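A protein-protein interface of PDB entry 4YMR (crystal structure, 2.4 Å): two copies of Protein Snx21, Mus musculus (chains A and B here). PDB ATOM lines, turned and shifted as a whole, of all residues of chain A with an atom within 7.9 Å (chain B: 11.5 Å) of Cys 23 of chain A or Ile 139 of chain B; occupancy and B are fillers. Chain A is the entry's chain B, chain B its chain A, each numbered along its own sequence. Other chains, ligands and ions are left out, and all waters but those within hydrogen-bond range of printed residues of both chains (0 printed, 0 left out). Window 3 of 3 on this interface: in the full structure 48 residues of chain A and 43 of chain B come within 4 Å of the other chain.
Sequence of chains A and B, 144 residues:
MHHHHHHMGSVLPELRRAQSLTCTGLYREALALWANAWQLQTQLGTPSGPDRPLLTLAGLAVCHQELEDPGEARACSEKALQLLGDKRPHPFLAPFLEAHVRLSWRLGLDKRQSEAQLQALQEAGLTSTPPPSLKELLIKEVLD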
ATOM      1  N   ARG A  17      19.191   8.262  24.588  1.00  0.00           N
ATOM      2  CA  ARG A  17      19.221   8.034  23.140  1.00  0.00           C
ATOM      3  C   ARG A  17      20.377   8.820  22.528  1.00  0.00           C
ATOM      4  O   ARG A  17      21.025   8.374  21.576  1.00  0.00           O
ATOM      5  CB  ARG A  17      17.886   8.472  22.514  1.00  0.00           C
ATOM      6  CG  ARG A  17      17.612   7.981  21.088  1.00  0.00           C
ATOM      7  CD  ARG A  17      16.312   8.587  20.519  1.00  0.00           C
ATOM      8  NE  ARG A  17      15.490   9.212  21.559  1.00  0.00           N
ATOM      9  CZ  ARG A  17      14.212   8.926  21.800  1.00  0.00           C
ATOM     10  NH1 ARG A  17      13.574   8.020  21.070  1.00  0.00           N
ATOM     11  NH2 ARG A  17      13.567   9.557  22.775  1.00  0.00           N
ATOM     12  N   ALA A  18      20.619  10.005  23.089  1.00  0.00           N
ATOM     13  CA  ALA A  18      21.746  10.845  22.705  1.00  0.00           C
ATOM     14  C   ALA A  18      23.072  10.214  23.141  1.00  0.00           C
ATOM     15  O   ALA A  18      24.023  10.151  22.357  1.00  0.00           O
ATOM     16  CB  ALA A  18      21.595  12.244  23.293  1.00  0.00           C
ATOM     17  N   GLN A  19      23.125   9.737  24.384  1.00  0.00           N
ATOM     18  CA  GLN A  19      24.314   9.061  24.909  1.00  0.00           C
ATOM     19  C   GLN A  19      24.748   7.845  24.079  1.00  0.00           C
ATOM     20  O   GLN A  19      25.939   7.623  23.855  1.00  0.00           O
ATOM     21  CB  GLN A  19      24.091   8.644  26.361  1.00  0.00           C
ATOM     22  CG  GLN A  19      25.281   7.964  27.014  1.00  0.00           C
ATOM     23  CD  GLN A  19      24.878   7.178  28.248  1.00  0.00           C
ATOM     24  OE1 GLN A  19      23.920   6.403  28.211  1.00  0.00           O
ATOM     25  NE2 GLN A  19      25.600   7.376  29.348  1.00  0.00           N
ATOM     26  N   SER A  20      23.783   7.064  23.608  1.00  0.00           N
ATOM     27  CA  SER A  20      24.113   5.842  22.885  1.00  0.00           C
ATOM     28  C   SER A  20      24.668   6.124  21.483  1.00  0.00           C
ATOM     29  O   SER A  20      25.537   5.392  20.999  1.00  0.00           O
ATOM     30  CB  SER A  20      22.922   4.864  22.850  1.00  0.00           C
ATOM     31  OG  SER A  20      21.966   5.219  21.871  1.00  0.00           O
ATOM     32  N   LEU A  21      24.178   7.182  20.839  1.00  0.00           N
ATOM     33  CA  LEU A  21      24.704   7.583  19.531  1.00  0.00           C
ATOM     34  C   LEU A  21      26.112   8.189  19.649  1.00  0.00           C
ATOM     35  O   LEU A  21      26.929   8.066  18.721  1.00  0.00           O
ATOM     36  CB  LEU A  21      23.745   8.551  18.810  1.00  0.00           C
ATOM     37  CG  LEU A  21      22.318   8.116  18.435  1.00  0.00           C
ATOM     38  CD1 LEU A  21      21.452   9.323  18.091  1.00  0.00           C
ATOM     39  CD2 LEU A  21      22.309   7.116  17.275  1.00  0.00           C
ATOM     40  N   THR A  22      26.377   8.838  20.787  1.00  0.00           N
ATOM     41  CA  THR A  22      27.683   9.452  21.083  1.00  0.00           C
ATOM     42  C   THR A  22      28.730   8.365  21.300  1.00  0.00           C
ATOM     43  O   THR A  22      29.851   8.446  20.781  1.00  0.00           O
ATOM     44  CB  THR A  22      27.611  10.412  22.312  1.00  0.00           C
ATOM     45  OG1 THR A  22      26.922  11.603  21.933  1.00  0.00           O
ATOM     46  CG2 THR A  22      28.984  10.812  22.794  1.00  0.00           C
ATOM     47  N   CYS A  23      28.340   7.336  22.049  1.00  0.00           N
ATOM     48  CA  CYS A  23      29.153   6.131  22.206  1.00  0.00           C
ATOM     49  C   CYS A  23      29.336   5.334  20.888  1.00  0.00           C
ATOM     50  O   CYS A  23      30.420   4.806  20.636  1.00  0.00           O
ATOM     51  CB  CYS A  23      28.598   5.250  23.342  1.00  0.00           C
ATOM     52  SG  CYS A  23      29.734   3.948  23.901  1.00  0.00           S
ATOM     53  N   THR A  24      28.298   5.273  20.047  1.00  0.00           N
ATOM     54  CA  THR A  24      28.380   4.663  18.696  1.00  0.00           C
ATOM     55  C   THR A  24      29.232   5.469  17.688  1.00  0.00           C
ATOM     56  O   THR A  24      29.668   4.955  16.653  1.00  0.00           O
ATOM     57  CB  THR A  24      26.954   4.430  18.101  1.00  0.00           C
ATOM     58  OG1 THR A  24      26.199   3.583  18.975  1.00  0.00           O
ATOM     59  CG2 THR A  24      26.998   3.786  16.724  1.00  0.00           C
ATOM     60  N   GLY A  25      29.476   6.740  17.991  1.00  0.00           N
ATOM     61  CA  GLY A  25      30.281   7.571  17.114  1.00  0.00           C
ATOM     62  C   GLY A  25      29.481   8.338  16.072  1.00  0.00           C
ATOM     63  O   GLY A  25      30.049   8.912  15.142  1.00  0.00           O
ATOM     64  N   LEU A  26      28.161   8.349  16.222  1.00  0.00           N
ATOM     65  CA  LEU A  26      27.293   9.082  15.303  1.00  0.00           C
ATOM     66  C   LEU A  26      27.033  10.461  15.907  1.00  0.00           C
ATOM     67  O   LEU A  26      26.064  10.670  16.626  1.00  0.00           O
ATOM     68  CB  LEU A  26      25.992   8.299  15.042  1.00  0.00           C
ATOM     69  CG  LEU A  26      26.148   6.906  14.401  1.00  0.00           C
ATOM     70  CD1 LEU A  26      24.888   6.065  14.558  1.00  0.00           C
ATOM     71  CD2 LEU A  26      26.555   7.002  12.927  1.00  0.00           C
ATOM     72  N   TYR A  27      27.912  11.410  15.622  1.00  0.00           N
ATOM     73  CA  TYR A  27      27.924  12.643  16.398  1.00  0.00           C
ATOM     74  C   TYR A  27      26.898  13.650  15.921  1.00  0.00           C
ATOM     75  O   TYR A  27      26.205  14.264  16.733  1.00  0.00           O
ATOM     76  CB  TYR A  27      29.326  13.248  16.443  1.00  0.00           C
ATOM     77  CG  TYR A  27      30.290  12.306  17.112  1.00  0.00           C
ATOM     78  CD1 TYR A  27      30.227  12.085  18.484  1.00  0.00           C
ATOM     79  CD2 TYR A  27      31.233  11.605  16.370  1.00  0.00           C
ATOM     80  CE1 TYR A  27      31.088  11.217  19.098  1.00  0.00           C
ATOM     81  CE2 TYR A  27      32.093  10.720  16.976  1.00  0.00           C
ATOM     82  CZ  TYR A  27      32.019  10.535  18.341  1.00  0.00           C
ATOM     83  OH  TYR A  27      32.880   9.665  18.955  1.00  0.00           O
ATOM     84  N   ALA A  30      23.588  12.487  17.236  1.00  0.00           N
ATOM     85  CA  ALA A  30      23.541  12.672  18.685  1.00  0.00           C
ATOM     86  C   ALA A  30      23.506  14.148  19.075  1.00  0.00           C
ATOM     87  O   ALA A  30      22.900  14.504  20.080  1.00  0.00           O
ATOM     88  CB  ALA A  30      24.719  11.979  19.351  1.00  0.00           C
ATOM     89  N   TRP A  34      21.063  15.989  21.664  1.00  0.00           N
ATOM     90  CA  TRP A  34      21.566  16.711  22.840  1.00  0.00           C
ATOM     91  C   TRP A  34      21.011  18.132  22.854  1.00  0.00           C
ATOM     92  O   TRP A  34      20.546  18.621  23.884  1.00  0.00           O
ATOM     93  CB  TRP A  34      23.100  16.779  22.880  1.00  0.00           C
ATOM     94  CG  TRP A  34      23.807  15.495  23.212  1.00  0.00           C
ATOM     95  CD1 TRP A  34      24.577  14.739  22.370  1.00  0.00           C
ATOM     96  CD2 TRP A  34      23.823  14.823  24.475  1.00  0.00           C
ATOM     97  NE1 TRP A  34      25.054  13.634  23.026  1.00  0.00           N
ATOM     98  CE2 TRP A  34      24.612  13.663  24.325  1.00  0.00           C
ATOM     99  CE3 TRP A  34      23.237  15.080  25.718  1.00  0.00           C
ATOM    100  CZ2 TRP A  34      24.832  12.764  25.364  1.00  0.00           C
ATOM    101  CZ3 TRP A  34      23.459  14.192  26.750  1.00  0.00           C
ATOM    102  CH2 TRP A  34      24.249  13.049  26.569  1.00  0.00           C
ATOM    103  N   LEU A  55      25.599  17.552  32.079  1.00  0.00           N
ATOM    104  CA  LEU A  55      25.723  16.382  31.212  1.00  0.00           C
ATOM    105  C   LEU A  55      25.284  16.665  29.786  1.00  0.00           C
ATOM    106  O   LEU A  55      25.876  16.141  28.835  1.00  0.00           O
ATOM    107  CB  LEU A  55      24.959  15.176  31.771  1.00  0.00           C
ATOM    108  CG  LEU A  55      25.251  13.864  31.023  1.00  0.00           C
ATOM    109  CD1 LEU A  55      25.907  12.879  31.956  1.00  0.00           C
ATOM    110  CD2 LEU A  55      24.017  13.254  30.348  1.00  0.00           C
ATOM    111  N   VAL A  62      31.234  17.492  23.521  1.00  0.00           N
ATOM    112  CA  VAL A  62      31.894  16.322  22.924  1.00  0.00           C
ATOM    113  C   VAL A  62      31.530  16.149  21.450  1.00  0.00           C
ATOM    114  O   VAL A  62      32.390  15.827  20.631  1.00  0.00           O
ATOM    115  CB  VAL A  62      31.637  15.021  23.728  1.00  0.00           C
ATOM    116  CG1 VAL A  62      31.880  13.774  22.873  1.00  0.00           C
ATOM    117  CG2 VAL A  62      32.508  14.997  24.971  1.00  0.00           C
ATOM    118  N   CYS A  63      30.273  16.412  21.106  1.00  0.00           N
ATOM    119  CA  CYS A  63      29.835  16.314  19.714  1.00  0.00           C
ATOM    120  C   CYS A  63      30.295  17.490  18.840  1.00  0.00           C
ATOM    121  O   CYS A  63      30.730  17.288  17.703  1.00  0.00           O
ATOM    122  CB  CYS A  63      28.318  16.126  19.625  1.00  0.00           C
ATOM    123  SG  CYS A  63      27.708  14.549  20.280  1.00  0.00           S
ATOM    124  N   SER B  48      30.394   9.496  43.411  1.00  0.00           N
ATOM    125  CA  SER B  48      30.378  10.181  42.124  1.00  0.00           C
ATOM    126  C   SER B  48      30.041  11.642  42.465  1.00  0.00           C
ATOM    127  O   SER B  48      30.772  12.283  43.216  1.00  0.00           O
ATOM    128  CB  SER B  48      29.405   9.587  41.111  1.00  0.00           C
ATOM    129  OG  SER B  48      29.974   9.585  39.818  1.00  0.00           O
ATOM    130  N   PHE B  92      32.472  16.761  37.090  1.00  0.00           N
ATOM    131  CA  PHE B  92      32.559  17.455  35.805  1.00  0.00           C
ATOM    132  C   PHE B  92      33.467  18.697  35.760  1.00  0.00           C
ATOM    133  O   PHE B  92      33.652  19.270  34.694  1.00  0.00           O
ATOM    134  CB  PHE B  92      31.164  17.818  35.303  1.00  0.00           C
ATOM    135  CG  PHE B  92      30.570  16.784  34.401  1.00  0.00           C
ATOM    136  CD1 PHE B  92      31.266  16.346  33.282  1.00  0.00           C
ATOM    137  CD2 PHE B  92      29.328  16.229  34.679  1.00  0.00           C
ATOM    138  CE1 PHE B  92      30.729  15.387  32.442  1.00  0.00           C
ATOM    139  CE2 PHE B  92      28.779  15.266  33.848  1.00  0.00           C
ATOM    140  CZ  PHE B  92      29.481  14.843  32.726  1.00  0.00           C
ATOM    141  N   PRO B  95      36.992  17.596  33.967  1.00  0.00           N
ATOM    142  CA  PRO B  95      36.805  17.329  32.534  1.00  0.00           C
ATOM    143  C   PRO B  95      36.521  18.577  31.704  1.00  0.00           C
ATOM    144  O   PRO B  95      36.954  18.661  30.547  1.00  0.00           O
ATOM    145  CB  PRO B  95      35.589  16.401  32.510  1.00  0.00           C
ATOM    146  CG  PRO B  95      35.595  15.738  33.814  1.00  0.00           C
ATOM    147  CD  PRO B  95      36.135  16.717  34.780  1.00  0.00           C
ATOM    148  N   PRO B 132      40.054  12.895  34.201  1.00  0.00           N
ATOM    149  CA  PRO B 132      39.080  12.167  33.377  1.00  0.00           C
ATOM    150  C   PRO B 132      38.593  13.071  32.264  1.00  0.00           C
ATOM    151  O   PRO B 132      38.708  14.287  32.371  1.00  0.00           O
ATOM    152  CB  PRO B 132      37.924  11.900  34.348  1.00  0.00           C
ATOM    153  CG  PRO B 132      38.533  11.943  35.685  1.00  0.00           C
ATOM    154  CD  PRO B 132      39.619  12.987  35.604  1.00  0.00           C
ATOM    155  N   SER B 133      38.058  12.507  31.197  1.00  0.00           N
ATOM    156  CA  SER B 133      37.674  13.368  30.096  1.00  0.00           C
ATOM    157  C   SER B 133      36.168  13.515  30.034  1.00  0.00           C
ATOM    158  O   SER B 133      35.429  12.759  30.668  1.00  0.00           O
ATOM    159  CB  SER B 133      38.239  12.877  28.763  1.00  0.00           C
ATOM    160  OG  SER B 133      37.495  11.785  28.281  1.00  0.00           O
ATOM    161  N   LEU B 134      35.736  14.510  29.265  1.00  0.00           N
ATOM    162  CA  LEU B 134      34.333  14.801  29.053  1.00  0.00           C
ATOM    163  C   LEU B 134      33.630  13.580  28.477  1.00  0.00           C
ATOM    164  O   LEU B 134      32.558  13.187  28.936  1.00  0.00           O
ATOM    165  CB  LEU B 134      34.218  16.007  28.128  1.00  0.00           C
ATOM    166  CG  LEU B 134      33.288  17.139  28.547  1.00  0.00           C
ATOM    167  CD1 LEU B 134      33.349  17.394  30.029  1.00  0.00           C
ATOM    168  CD2 LEU B 134      33.630  18.393  27.775  1.00  0.00           C
ATOM    169  N   LYS B 135      34.274  12.967  27.493  1.00  0.00           N
ATOM    170  CA  LYS B 135      33.775  11.768  26.829  1.00  0.00           C
ATOM    171  C   LYS B 135      33.735  10.545  27.758  1.00  0.00           C
ATOM    172  O   LYS B 135      32.772   9.773  27.729  1.00  0.00           O
ATOM    173  CB  LYS B 135      34.637  11.485  25.600  1.00  0.00           C
ATOM    174  CG  LYS B 135      33.990  10.608  24.535  1.00  0.00           C
ATOM    175  CD  LYS B 135      34.641  10.875  23.173  1.00  0.00           C
ATOM    176  CE  LYS B 135      33.994  10.055  22.072  1.00  0.00           C
ATOM    177  NZ  LYS B 135      34.826  10.043  20.831  1.00  0.00           N
ATOM    178  N   GLU B 136      34.781  10.370  28.568  1.00  0.00           N
ATOM    179  CA  GLU B 136      34.831   9.288  29.558  1.00  0.00           C
ATOM    180  C   GLU B 136      33.627   9.334  30.498  1.00  0.00           C
ATOM    181  O   GLU B 136      32.916   8.344  30.666  1.00  0.00           O
ATOM    182  CB  GLU B 136      36.126   9.341  30.382  1.00  0.00           C
ATOM    183  CG  GLU B 136      36.176   8.322  31.531  1.00  0.00           C
ATOM    184  CD  GLU B 136      37.477   8.381  32.344  1.00  0.00           C
ATOM    185  OE1 GLU B 136      38.428   9.067  31.905  1.00  0.00           O
ATOM    186  OE2 GLU B 136      37.546   7.744  33.424  1.00  0.00           O
ATOM    187  N   LEU B 137      33.407  10.493  31.107  1.00  0.00           N
ATOM    188  CA  LEU B 137      32.309  10.659  32.056  1.00  0.00           C
ATOM    189  C   LEU B 137      30.962  10.594  31.356  1.00  0.00           C
ATOM    190  O   LEU B 137      29.982  10.117  31.923  1.00  0.00           O
ATOM    191  CB  LEU B 137      32.453  11.967  32.829  1.00  0.00           C
ATOM    192  CG  LEU B 137      33.163  11.807  34.172  1.00  0.00           C
ATOM    193  CD1 LEU B 137      34.547  11.260  33.971  1.00  0.00           C
ATOM    194  CD2 LEU B 137      33.224  13.128  34.913  1.00  0.00           C
ATOM    195  N   LEU B 138      30.930  11.054  30.111  1.00  0.00           N
ATOM    196  CA  LEU B 138      29.730  10.965  29.297  1.00  0.00           C
ATOM    197  C   LEU B 138      29.207   9.535  29.186  1.00  0.00           C
ATOM    198  O   LEU B 138      28.057   9.268  29.520  1.00  0.00           O
ATOM    199  CB  LEU B 138      29.979  11.542  27.910  1.00  0.00           C
ATOM    200  CG  LEU B 138      28.714  11.910  27.142  1.00  0.00           C
ATOM    201  CD1 LEU B 138      27.804  12.790  28.022  1.00  0.00           C
ATOM    202  CD2 LEU B 138      29.084  12.623  25.851  1.00  0.00           C
ATOM    203  N   ILE B 139      30.057   8.612  28.741  1.00  0.00           N
ATOM    204  CA  ILE B 139      29.641   7.218  28.545  1.00  0.00           C
ATOM    205  C   ILE B 139      29.468   6.412  29.849  1.00  0.00           C
ATOM    206  O   ILE B 139      28.608   5.534  29.932  1.00  0.00           O
ATOM    207  CB  ILE B 139      30.579   6.469  27.563  1.00  0.00           C
ATOM    208  CG1 ILE B 139      31.995   6.370  28.138  1.00  0.00           C
ATOM    209  CG2 ILE B 139      30.586   7.146  26.185  1.00  0.00           C
ATOM    210  CD1 ILE B 139      32.354   4.999  28.662  1.00  0.00           C
ATOM    211  N   LYS B 140      30.278   6.708  30.863  1.00  0.00           N
ATOM    212  CA  LYS B 140      30.226   5.963  32.125  1.00  0.00           C
ATOM    213  C   LYS B 140      29.033   6.335  32.992  1.00  0.00           C
ATOM    214  O   LYS B 140      28.663   5.588  33.897  1.00  0.00           O
ATOM    215  CB  LYS B 140      31.527   6.122  32.918  1.00  0.00           C
ATOM    216  CG  LYS B 140      32.505   4.974  32.693  1.00  0.00           C
ATOM    217  CD  LYS B 140      33.927   5.321  33.100  1.00  0.00           C
ATOM    218  CE  LYS B 140      34.915   4.537  32.248  1.00  0.00           C
ATOM    219  NZ  LYS B 140      36.340   4.798  32.594  1.00  0.00           N
ATOM    220  N   GLU B 141      28.440   7.491  32.715  1.00  0.00           N
ATOM    221  CA  GLU B 141      27.248   7.922  33.428  1.00  0.00           C
ATOM    222  C   GLU B 141      26.071   6.987  33.144  1.00  0.00           C
ATOM    223  O   GLU B 141      25.744   6.721  31.981  1.00  0.00           O
ATOM    224  CB  GLU B 141      26.883   9.340  33.013  1.00  0.00           C
ATOM    225  CG  GLU B 141      25.606   9.836  33.650  1.00  0.00           C
ATOM    226  CD  GLU B 141      25.807  10.267  35.080  1.00  0.00           C
ATOM    227  OE1 GLU B 141      26.910  10.748  35.403  1.00  0.00           O
ATOM    228  OE2 GLU B 141      24.865  10.120  35.884  1.00  0.00           O
ATOM    229  N   VAL B 142      25.439   6.485  34.204  1.00  0.00           N
ATOM    230  CA  VAL B 142      24.273   5.625  34.056  1.00  0.00           C
ATOM    231  C   VAL B 142      22.990   6.454  34.040  1.00  0.00           C
ATOM    232  O   VAL B 142      22.768   7.279  34.927  1.00  0.00           O
ATOM    233  CB  VAL B 142      24.180   4.583  35.194  1.00  0.00           C
ATOM    234  CG1 VAL B 142      23.202   3.476  34.812  1.00  0.00           C
ATOM    235  CG2 VAL B 142      25.547   3.998  35.512  1.00  0.00           C
ATOM    236  N   LEU B 143      22.151   6.232  33.029  1.00  0.00           N
ATOM    237  CA  LEU B 143      20.860   6.922  32.923  1.00  0.00           C
ATOM    238  C   LEU B 143      19.714   5.954  33.283  1.00  0.00           C
ATOM    239  O   LEU B 143      19.086   5.342  32.423  1.00  0.00           O
ATOM    240  CB  LEU B 143      20.708   7.568  31.543  1.00  0.00           C
ATOM    241  CG  LEU B 143      21.828   8.587  31.292  1.00  0.00           C
ATOM    242  CD1 LEU B 143      21.975   9.028  29.825  1.00  0.00           C
ATOM    243  CD2 LEU B 143      21.641   9.795  32.199  1.00  0.00           C
ATOM    244  N   ASP B 144      19.433   5.884  34.583  1.00  0.00           N
ATOM    245  CA  ASP B 144      19.001   4.655  35.264  1.00  0.00           C
ATOM    246  C   ASP B 144      17.560   4.168  35.056  1.00  0.00           C
ATOM    247  O   ASP B 144      16.633   4.956  34.862  1.00  0.00           O
ATOM    248  CB  ASP B 144      19.331   4.752  36.770  1.00  0.00           C
ATOM    249  CG  ASP B 144      20.249   3.627  37.236  1.00  0.00           C
ATOM    250  OD1 ASP B 144      20.288   2.580  36.545  1.00  0.00           O
ATOM    251  OD2 ASP B 144      20.925   3.776  38.283  1.00  0.00           O
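No position is printed for both chains. Of the 12 pairs that touch across the chains among the printed residues, none has its exchanged pair printed and touching as well.
Among the printed residues, merely in contact across the chains: Leu 55 of chain A with Glu 141 of chain B (3.5 Å), Thr 22 of chain A with Leu 138 of chain B (3.6 Å), Gln 19 of chain A with Ile 139 of chain B (3.6 Å), Gln 19 of chain A with Leu 143 of chain B (3.6 Å), Val 62 of chain A with Lys 135 of chain B (3.7 Å), Val 62 of chain A with Leu 134 of chain B (3.7 Å), Trp 34 of chain A with Leu 138 of chain B (3.8 Å), Leu 55 of chain A with Leu 138 of chain B (3.95 Å) and Cys 23 of chain A with Ile 139 of chain B (3.95 Å).
Of chain B, only Ile 139 comes within 4 Å of Cys 23 of chain A. Of chain A, only Gln 19 (3.6 Å) and Cys 23 (3.95 Å) come within 4 Å of Ile 139 of chain B. Thr 22 of chain A touches just one residue of chain B: Leu 138 (3.6 Å). Thr 24 of chain A touches none of the printed residues of chain B. No residue of chain B comes within 4 Å of Gly 25 of chain A. Printed residues of chain A within 4 Å of Leu 138 of chain B: Gln 19 (3.1 Å), Thr 22 (3.6 Å), Trp 34 (3.8 Å) and Leu 55 (3.95 Å). Of the printed residues of chain A, Glu 141 of chain B touches Gln 19 (2.7 Å) and Leu 55 (3.5 Å). Leu 26 of chain A touches none of the printed residues of chain B. The nearest residue of chain B that does not touch Cys 23 of chain A is Lys 135 of chain B (6.2 Å). The nearest residue of chain A that does not touch Ile 139 of chain B is Thr 22 of chain A (5.2 Å).
Along chain B the printed residues that touch a printed residue of chain A span positions 134 to 143. Hydrophobic or aromatic side chains of chain A within 4 Å of the printed part of chain B: Tyr 27, Trp 34, Leu 55 and Val 62. Among the printed residues, 12 pairs touch across the chains. Among the printed residues, no Asp or Glu carboxylate lies within 4 Å of a Lys or Arg side-chain nitrogen of the other chain.
OH of Tyr 27 of chain A is in hydrogen-bond range of NZ of Lys 135 of chain B. O of Leu 138 of chain B is in hydrogen-bond range of NE2 of Gln 19 of chain A, at 3.1 Å. NE2 of Gln 19 of chain A sits at hydrogen-bond distance from O of Glu 141 of chain B (2.7 Å).
The backbone carbonyl oxygen (O) of Ala 18 of chain A sits at hydrogen-bond distance from the side-chain hydroxyl (OG1) of Thr 22 of chain A (3.3 Å). The side-chain hydroxyl (OG1) of Thr 22 of chain A sits at hydrogen-bond distance from the indole nitrogen (NE1) of Trp 34 of chain A (3.0 Å). The side-chain hydroxyl of Thr 22 of chain A lies within hydrogen-bond range of the side-chain sulfur of Cys 63 of chain A, 3.5 Å away.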
